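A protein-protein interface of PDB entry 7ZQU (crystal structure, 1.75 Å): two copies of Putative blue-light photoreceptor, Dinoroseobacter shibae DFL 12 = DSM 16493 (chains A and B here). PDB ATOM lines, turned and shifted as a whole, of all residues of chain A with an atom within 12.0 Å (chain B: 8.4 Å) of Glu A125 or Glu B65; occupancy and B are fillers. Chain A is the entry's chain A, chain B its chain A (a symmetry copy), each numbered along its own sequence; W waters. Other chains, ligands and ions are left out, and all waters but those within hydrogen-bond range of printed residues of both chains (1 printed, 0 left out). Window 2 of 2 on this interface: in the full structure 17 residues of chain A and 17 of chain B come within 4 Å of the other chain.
The backbone NH (N) of Met A129 lies within hydrogen-bond range of the backbone carbonyl oxygen (O) of Ile A121. The side-chain carboxylate (OD1) of Asp A123 lies within hydrogen-bond range of the backbone NH (N) of Glu A125, at 2.8 Å. The side-chain carboxylate (OD1) of Asp A123 sits at hydrogen-bond distance from the backbone NH (N) of Gly A126 (2.9 Å). N of Asn A127 sits at hydrogen-bond distance from OD1 of Asp A123 (2.8 Å).
Along chain B the printed residues that touch a printed residue of chain A span positions 50 to 68. Hydrophobic or aromatic side chains of chain A within 4 Å of the printed part of chain B: Pro A124 and Met A129. Among the printed residues, 6 pairs touch across the chains. Among the printed residues, no Asp or Glu carboxylate lies within 4 Å of a Lys or Arg side-chain nitrogen of the other chain.
Water W1 bridges the side-chain carboxylate of Asp A123 and the backbone carbonyl oxygen of Ile B50.
Of the printed residues of chain B, Glu A125 touches Glu B65 and Leu B68. Of the printed residues of chain A, Glu B65 touches Glu A125. No residue of chain B comes within 4 Å of Gly A126. No residue of chain A comes within 4 Å of Glu B66. No residue of chain A comes within 4 Å of Val B67. Of chain A, only Asp A123 (3.4 Å) and Glu A125 (3.6 Å) come within 4 Å of Leu B68. Of the printed residues of chain B, Asp A123 touches Ile B50 and Leu B68. Printed residues of chain A within 4 Å of Ile B50: Asp A123 and Met A129. Of the printed residues of chain B, Met A129 touches Ile B50. Printed residues of chain A within 4 Å of Leu B64: Pro A124 (3.6 Å). The nearest residue of chain A that does not touch Glu B65 is Asn A127 (7.1 Å).
OE2 of Glu B65 sits close to OE2 of Glu A125, 3.3 Å away.
Ile B50 touches Asp A123. CD1 of Leu B68 touches OD2 of Asp A123, at 3.4 Å. O of Pro A124 touches CD1 of Leu B64, at 3.6 Å. Leu B68 touches Glu A125. Met A129 touches Ile B50.
No position is printed for both chains. Of the 6 pairs that touch across the chains among the printed residues, none has its exchanged pair printed and touching as well.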
ATOM      1  N   GLU A  95      12.383  -4.658   2.166  1.00  0.00           N
ATOM      2  CA  GLU A  95      12.235  -5.844   3.011  1.00  0.00           C
ATOM      3  C   GLU A  95      12.717  -5.573   4.433  1.00  0.00           C
ATOM      4  O   GLU A  95      13.570  -6.276   4.973  1.00  0.00           O
ATOM      5  CB  GLU A  95      12.971  -7.041   2.419  1.00  0.00           C
ATOM      6  CG  GLU A  95      12.534  -7.398   1.033  1.00  0.00           C
ATOM      7  CD  GLU A  95      13.222  -8.649   0.511  1.00  0.00           C
ATOM      8  OE1 GLU A  95      14.042  -9.256   1.242  1.00  0.00           O
ATOM      9  OE2 GLU A  95      12.919  -9.028  -0.636  1.00  0.00           O
ATOM     10  N   PRO A 120       8.539  -7.769   7.216  1.00  0.00           N
ATOM     11  CA  PRO A 120       8.686  -8.977   6.401  1.00  0.00           C
ATOM     12  C   PRO A 120       8.585 -10.216   7.275  1.00  0.00           C
ATOM     13  O   PRO A 120       8.972 -10.204   8.446  1.00  0.00           O
ATOM     14  CB  PRO A 120      10.089  -8.831   5.800  1.00  0.00           C
ATOM     15  CG  PRO A 120      10.829  -7.964   6.776  1.00  0.00           C
ATOM     16  CD  PRO A 120       9.802  -7.008   7.327  1.00  0.00           C
ATOM     17  N   ILE A 121       8.072 -11.297   6.687  1.00  0.00           N
ATOM     18  CA  ILE A 121       8.014 -12.608   7.322  1.00  0.00           C
ATOM     19  C   ILE A 121       8.961 -13.516   6.559  1.00  0.00           C
ATOM     20  O   ILE A 121       8.779 -13.729   5.355  1.00  0.00           O
ATOM     21  CB  ILE A 121       6.595 -13.198   7.316  1.00  0.00           C
ATOM     22  CG1 ILE A 121       5.605 -12.229   7.969  1.00  0.00           C
ATOM     23  CG2 ILE A 121       6.591 -14.527   8.033  1.00  0.00           C
ATOM     24  CD1 ILE A 121       5.868 -12.007   9.437  1.00  0.00           C
ATOM     25  N   TYR A 122       9.965 -14.059   7.244  1.00  0.00           N
ATOM     26  CA  TYR A 122      11.017 -14.801   6.570  1.00  0.00           C
ATOM     27  C   TYR A 122      10.859 -16.302   6.739  1.00  0.00           C
ATOM     28  O   TYR A 122      10.331 -16.788   7.742  1.00  0.00           O
ATOM     29  CB  TYR A 122      12.393 -14.398   7.092  1.00  0.00           C
ATOM     30  CG  TYR A 122      12.780 -12.990   6.745  1.00  0.00           C
ATOM     31  CD1 TYR A 122      13.222 -12.668   5.466  1.00  0.00           C
ATOM     32  CD2 TYR A 122      12.716 -11.979   7.695  1.00  0.00           C
ATOM     33  CE1 TYR A 122      13.594 -11.369   5.148  1.00  0.00           C
ATOM     34  CE2 TYR A 122      13.085 -10.684   7.390  1.00  0.00           C
ATOM     35  CZ  TYR A 122      13.521 -10.384   6.117  1.00  0.00           C
ATOM     36  OH  TYR A 122      13.883  -9.090   5.814  1.00  0.00           O
ATOM     37  N   ASP A 123      11.346 -17.039   5.754  1.00  0.00           N
ATOM     38  CA  ASP A 123      11.443 -18.478   5.890  1.00  0.00           C
ATOM     39  C   ASP A 123      12.653 -18.793   6.764  1.00  0.00           C
ATOM     40  O   ASP A 123      13.414 -17.894   7.130  1.00  0.00           O
ATOM     41  CB  ASP A 123      11.471 -19.123   4.497  1.00  0.00           C
ATOM     42  CG  ASP A 123      12.790 -18.941   3.751  1.00  0.00           C
ATOM     43  OD1 ASP A 123      13.795 -18.479   4.329  1.00  0.00           O
ATOM     44  OD2 ASP A 123      12.802 -19.296   2.550  1.00  0.00           O
ATOM     45  N   PRO A 124      12.862 -20.061   7.138  1.00  0.00           N
ATOM     46  CA  PRO A 124      13.969 -20.366   8.058  1.00  0.00           C
ATOM     47  C   PRO A 124      15.342 -20.062   7.487  1.00  0.00           C
ATOM     48  O   PRO A 124      16.315 -20.041   8.250  1.00  0.00           O
ATOM     49  CB  PRO A 124      13.803 -21.868   8.328  1.00  0.00           C
ATOM     50  CG  PRO A 124      12.388 -22.181   7.979  1.00  0.00           C
ATOM     51  CD  PRO A 124      12.045 -21.258   6.861  1.00  0.00           C
ATOM     52  N   GLU A 125      15.448 -19.832   6.182  1.00  0.00           N
ATOM     53  CA  GLU A 125      16.713 -19.570   5.507  1.00  0.00           C
ATOM     54  C   GLU A 125      16.934 -18.083   5.248  1.00  0.00           C
ATOM     55  O   GLU A 125      17.957 -17.705   4.676  1.00  0.00           O
ATOM     56  CB  GLU A 125      16.755 -20.382   4.194  1.00  0.00           C
ATOM     57  CG  GLU A 125      17.981 -20.259   3.273  1.00  0.00           C
ATOM     58  CD  GLU A 125      19.274 -20.512   3.967  1.00  0.00           C
ATOM     59  OE1 GLU A 125      19.252 -20.994   5.119  1.00  0.00           O
ATOM     60  OE2 GLU A 125      20.335 -20.236   3.355  1.00  0.00           O
ATOM     61  N   GLY A 126      16.016 -17.230   5.684  1.00  0.00           N
ATOM     62  CA  GLY A 126      16.148 -15.802   5.493  1.00  0.00           C
ATOM     63  C   GLY A 126      15.539 -15.253   4.223  1.00  0.00           C
ATOM     64  O   GLY A 126      15.720 -14.063   3.940  1.00  0.00           O
ATOM     65  N   ASN A 127      14.841 -16.076   3.441  1.00  0.00           N
ATOM     66  CA  ASN A 127      14.153 -15.595   2.254  1.00  0.00           C
ATOM     67  C   ASN A 127      12.812 -14.981   2.637  1.00  0.00           C
ATOM     68  O   ASN A 127      12.136 -15.438   3.565  1.00  0.00           O
ATOM     69  CB  ASN A 127      13.913 -16.727   1.255  1.00  0.00           C
ATOM     70  CG  ASN A 127      15.164 -17.420   0.852  1.00  0.00           C
ATOM     71  OD1 ASN A 127      16.117 -16.786   0.400  1.00  0.00           O
ATOM     72  ND2 ASN A 127      15.183 -18.737   1.008  1.00  0.00           N
ATOM     73  N   LEU A 128      12.428 -13.939   1.907  1.00  0.00           N
ATOM     74  CA  LEU A 128      11.134 -13.307   2.127  1.00  0.00           C
ATOM     75  C   LEU A 128      10.008 -14.263   1.748  1.00  0.00           C
ATOM     76  O   LEU A 128       9.984 -14.794   0.631  1.00  0.00           O
ATOM     77  CB  LEU A 128      11.044 -12.031   1.303  1.00  0.00           C
ATOM     78  CG  LEU A 128       9.774 -11.198   1.461  1.00  0.00           C
ATOM     79  CD1 LEU A 128       9.746 -10.631   2.854  1.00  0.00           C
ATOM     80  CD2 LEU A 128       9.742 -10.094   0.428  1.00  0.00           C
ATOM     81  N   MET A 129       9.082 -14.497   2.683  1.00  0.00           N
ATOM     82  CA  MET A 129       7.893 -15.308   2.435  1.00  0.00           C
ATOM     83  C   MET A 129       6.676 -14.431   2.196  1.00  0.00           C
ATOM     84  O   MET A 129       6.029 -14.518   1.147  1.00  0.00           O
ATOM     85  CB  MET A 129       7.551 -16.227   3.618  1.00  0.00           C
ATOM     86  CG  MET A 129       8.530 -17.286   4.005  1.00  0.00           C
ATOM     87  SD  MET A 129       7.702 -18.518   5.050  1.00  0.00           S
ATOM     88  CE  MET A 129       6.621 -19.266   3.860  1.00  0.00           C
ATOM     89  N   PHE A 130       6.339 -13.613   3.192  1.00  0.00           N
ATOM     90  CA  PHE A 130       5.183 -12.735   3.165  1.00  0.00           C
ATOM     91  C   PHE A 130       5.573 -11.391   3.755  1.00  0.00           C
ATOM     92  O   PHE A 130       6.598 -11.255   4.432  1.00  0.00           O
ATOM     93  CB  PHE A 130       4.010 -13.288   3.988  1.00  0.00           C
ATOM     94  CG  PHE A 130       3.767 -14.749   3.813  1.00  0.00           C
ATOM     95  CD1 PHE A 130       3.320 -15.248   2.603  1.00  0.00           C
ATOM     96  CD2 PHE A 130       3.936 -15.620   4.875  1.00  0.00           C
ATOM     97  CE1 PHE A 130       3.067 -16.595   2.438  1.00  0.00           C
ATOM     98  CE2 PHE A 130       3.695 -16.969   4.721  1.00  0.00           C
ATOM     99  CZ  PHE A 130       3.249 -17.462   3.496  1.00  0.00           C
ATOM    100  N   ILE B  50       7.671 -23.680   0.239  1.00  0.00           N
ATOM    101  CA  ILE B  50       8.001 -22.391   0.844  1.00  0.00           C
ATOM    102  C   ILE B  50       8.304 -22.507   2.323  1.00  0.00           C
ATOM    103  O   ILE B  50       8.788 -21.534   2.923  1.00  0.00           O
ATOM    104  CB  ILE B  50       6.877 -21.356   0.628  1.00  0.00           C
ATOM    105  CG1 ILE B  50       5.546 -21.920   1.143  1.00  0.00           C
ATOM    106  CG2 ILE B  50       6.811 -20.945  -0.840  1.00  0.00           C
ATOM    107  CD1 ILE B  50       4.447 -20.875   1.375  1.00  0.00           C
ATOM    108  N   TYR B  51       8.007 -23.641   2.936  1.00  0.00           N
ATOM    109  CA  TYR B  51       8.295 -23.866   4.337  1.00  0.00           C
ATOM    110  C   TYR B  51       8.446 -25.363   4.532  1.00  0.00           C
ATOM    111  O   TYR B  51       7.657 -26.139   3.987  1.00  0.00           O
ATOM    112  CB  TYR B  51       7.193 -23.335   5.255  1.00  0.00           C
ATOM    113  CG  TYR B  51       7.362 -23.819   6.669  1.00  0.00           C
ATOM    114  CD1 TYR B  51       8.158 -23.114   7.563  1.00  0.00           C
ATOM    115  CD2 TYR B  51       6.765 -25.009   7.107  1.00  0.00           C
ATOM    116  CE1 TYR B  51       8.346 -23.560   8.860  1.00  0.00           C
ATOM    117  CE2 TYR B  51       6.944 -25.467   8.406  1.00  0.00           C
ATOM    118  CZ  TYR B  51       7.737 -24.737   9.275  1.00  0.00           C
ATOM    119  OH  TYR B  51       7.935 -25.167  10.575  1.00  0.00           O
ATOM    120  N   VAL B  52       9.457 -25.770   5.307  1.00  0.00           N
ATOM    121  CA  VAL B  52       9.607 -27.164   5.726  1.00  0.00           C
ATOM    122  C   VAL B  52       9.881 -27.176   7.227  1.00  0.00           C
ATOM    123  O   VAL B  52      10.579 -26.300   7.748  1.00  0.00           O
ATOM    124  CB  VAL B  52      10.721 -27.908   4.945  1.00  0.00           C
ATOM    125  CG1 VAL B  52      10.498 -27.788   3.444  1.00  0.00           C
ATOM    126  CG2 VAL B  52      12.096 -27.354   5.282  1.00  0.00           C
ATOM    127  N   LEU B  57      13.629 -31.749   7.558  1.00  0.00           N
ATOM    128  CA  LEU B  57      15.042 -31.634   7.205  1.00  0.00           C
ATOM    129  C   LEU B  57      15.858 -32.752   7.838  1.00  0.00           C
ATOM    130  O   LEU B  57      16.698 -33.379   7.179  1.00  0.00           O
ATOM    131  CB  LEU B  57      15.584 -30.275   7.643  1.00  0.00           C
ATOM    132  CG  LEU B  57      14.974 -29.047   6.974  1.00  0.00           C
ATOM    133  CD1 LEU B  57      15.379 -27.795   7.709  1.00  0.00           C
ATOM    134  CD2 LEU B  57      15.382 -28.968   5.512  1.00  0.00           C
ATOM    135  N   TYR B  62      18.577 -33.351   4.540  1.00  0.00           N
ATOM    136  CA  TYR B  62      18.876 -32.172   3.730  1.00  0.00           C
ATOM    137  C   TYR B  62      19.024 -30.916   4.591  1.00  0.00           C
ATOM    138  O   TYR B  62      18.522 -30.840   5.714  1.00  0.00           O
ATOM    139  CB  TYR B  62      17.780 -31.910   2.692  1.00  0.00           C
ATOM    140  CG  TYR B  62      17.740 -32.888   1.549  1.00  0.00           C
ATOM    141  CD1 TYR B  62      18.653 -32.802   0.510  1.00  0.00           C
ATOM    142  CD2 TYR B  62      16.786 -33.897   1.510  1.00  0.00           C
ATOM    143  CE1 TYR B  62      18.630 -33.699  -0.539  1.00  0.00           C
ATOM    144  CE2 TYR B  62      16.749 -34.813   0.458  1.00  0.00           C
ATOM    145  CZ  TYR B  62      17.668 -34.706  -0.561  1.00  0.00           C
ATOM    146  OH  TYR B  62      17.654 -35.597  -1.612  1.00  0.00           O
ATOM    147  N   THR B  63      19.716 -29.919   4.034  1.00  0.00           N
ATOM    148  CA  THR B  63      19.769 -28.581   4.606  1.00  0.00           C
ATOM    149  C   THR B  63      18.699 -27.708   3.954  1.00  0.00           C
ATOM    150  O   THR B  63      18.199 -28.010   2.867  1.00  0.00           O
ATOM    151  CB  THR B  63      21.150 -27.948   4.405  1.00  0.00           C
ATOM    152  OG1 THR B  63      21.412 -27.849   3.003  1.00  0.00           O
ATOM    153  CG2 THR B  63      22.239 -28.807   5.036  1.00  0.00           C
ATOM    154  N   LEU B  64      18.352 -26.612   4.632  1.00  0.00           N
ATOM    155  CA  LEU B  64      17.356 -25.684   4.093  1.00  0.00           C
ATOM    156  C   LEU B  64      17.708 -25.250   2.672  1.00  0.00           C
ATOM    157  O   LEU B  64      16.844 -25.219   1.785  1.00  0.00           O
ATOM    158  CB  LEU B  64      17.239 -24.453   4.998  1.00  0.00           C
ATOM    159  CG  LEU B  64      16.486 -24.590   6.316  1.00  0.00           C
ATOM    160  CD1 LEU B  64      16.884 -23.486   7.302  1.00  0.00           C
ATOM    161  CD2 LEU B  64      15.006 -24.565   6.033  1.00  0.00           C
ATOM    162  N   GLU B  65      18.977 -24.899   2.442  1.00  0.00           N
ATOM    163  CA  GLU B  65      19.391 -24.414   1.127  1.00  0.00           C
ATOM    164  C   GLU B  65      19.092 -25.418   0.025  1.00  0.00           C
ATOM    165  O   GLU B  65      18.862 -25.025  -1.123  1.00  0.00           O
ATOM    166  CB  GLU B  65      20.882 -24.082   1.124  1.00  0.00           C
ATOM    167  CG  GLU B  65      21.217 -22.733   1.696  1.00  0.00           C
ATOM    168  CD  GLU B  65      22.657 -22.306   1.386  1.00  0.00           C
ATOM    169  OE1 GLU B  65      23.312 -22.992   0.560  1.00  0.00           O
ATOM    170  OE2 GLU B  65      23.129 -21.290   1.962  1.00  0.00           O
ATOM    171  N   GLU B  66      19.093 -26.707   0.347  1.00  0.00           N
ATOM    172  CA  GLU B  66      18.888 -27.742  -0.653  1.00  0.00           C
ATOM    173  C   GLU B  66      17.424 -27.988  -0.994  1.00  0.00           C
ATOM    174  O   GLU B  66      17.148 -28.709  -1.957  1.00  0.00           O
ATOM    175  CB  GLU B  66      19.514 -29.053  -0.175  1.00  0.00           C
ATOM    176  CG  GLU B  66      21.032 -28.987  -0.042  1.00  0.00           C
ATOM    177  CD  GLU B  66      21.612 -30.238   0.592  1.00  0.00           C
ATOM    178  OE1 GLU B  66      21.516 -30.378   1.830  1.00  0.00           O
ATOM    179  OE2 GLU B  66      22.156 -31.079  -0.152  1.00  0.00           O
ATOM    180  N   VAL B  67      16.475 -27.427  -0.251  1.00  0.00           N
ATOM    181  CA  VAL B  67      15.090 -27.842  -0.470  1.00  0.00           C
ATOM    182  C   VAL B  67      14.149 -26.654  -0.653  1.00  0.00           C
ATOM    183  O   VAL B  67      13.125 -26.768  -1.338  1.00  0.00           O
ATOM    184  CB  VAL B  67      14.592 -28.747   0.674  1.00  0.00           C
ATOM    185  CG1 VAL B  67      15.526 -29.928   0.886  1.00  0.00           C
ATOM    186  CG2 VAL B  67      14.425 -27.968   1.955  1.00  0.00           C
ATOM    187  N   LEU B  68      14.451 -25.518  -0.032  1.00  0.00           N
ATOM    188  CA  LEU B  68      13.515 -24.406  -0.130  1.00  0.00           C
ATOM    189  C   LEU B  68      13.500 -23.866  -1.549  1.00  0.00           C
ATOM    190  O   LEU B  68      14.549 -23.693  -2.175  1.00  0.00           O
ATOM    191  CB  LEU B  68      13.872 -23.301   0.851  1.00  0.00           C
ATOM    192  CG  LEU B  68      13.475 -23.563   2.304  1.00  0.00           C
ATOM    193  CD1 LEU B  68      13.934 -22.398   3.187  1.00  0.00           C
ATOM    194  CD2 LEU B  68      11.967 -23.786   2.432  1.00  0.00           C
ATOM    195  N   GLY B  69      12.296 -23.601  -2.055  1.00  0.00           N
ATOM    196  CA  GLY B  69      12.148 -23.153  -3.421  1.00  0.00           C
ATOM    197  C   GLY B  69      12.105 -24.255  -4.455  1.00  0.00           C
ATOM    198  O   GLY B  69      12.071 -23.956  -5.653  1.00  0.00           O
ATOM    199  N   ARG B  70      12.105 -25.519  -4.036  1.00  0.00           N
ATOM    200  CA  ARG B  70      12.072 -26.651  -4.943  1.00  0.00           C
ATOM    201  C   ARG B  70      10.786 -27.436  -4.742  1.00  0.00           C
ATOM    202  O   ARG B  70      10.254 -27.510  -3.631  1.00  0.00           O
ATOM    203  CB  ARG B  70      13.256 -27.595  -4.704  1.00  0.00           C
ATOM    204  CG  ARG B  70      14.603 -27.000  -5.040  1.00  0.00           C
ATOM    205  CD  ARG B  70      15.706 -27.999  -4.717  1.00  0.00           C
ATOM    206  NE  ARG B  70      15.630 -29.189  -5.553  1.00  0.00           N
ATOM    207  CZ  ARG B  70      16.144 -30.364  -5.214  1.00  0.00           C
ATOM    208  NH1 ARG B  70      16.718 -30.549  -4.037  1.00  0.00           N
ATOM    209  NH2 ARG B  70      16.084 -31.377  -6.076  1.00  0.00           N
HETATM  210  O   HOH W   1      10.373 -19.792   1.203  1.00  0.00           O
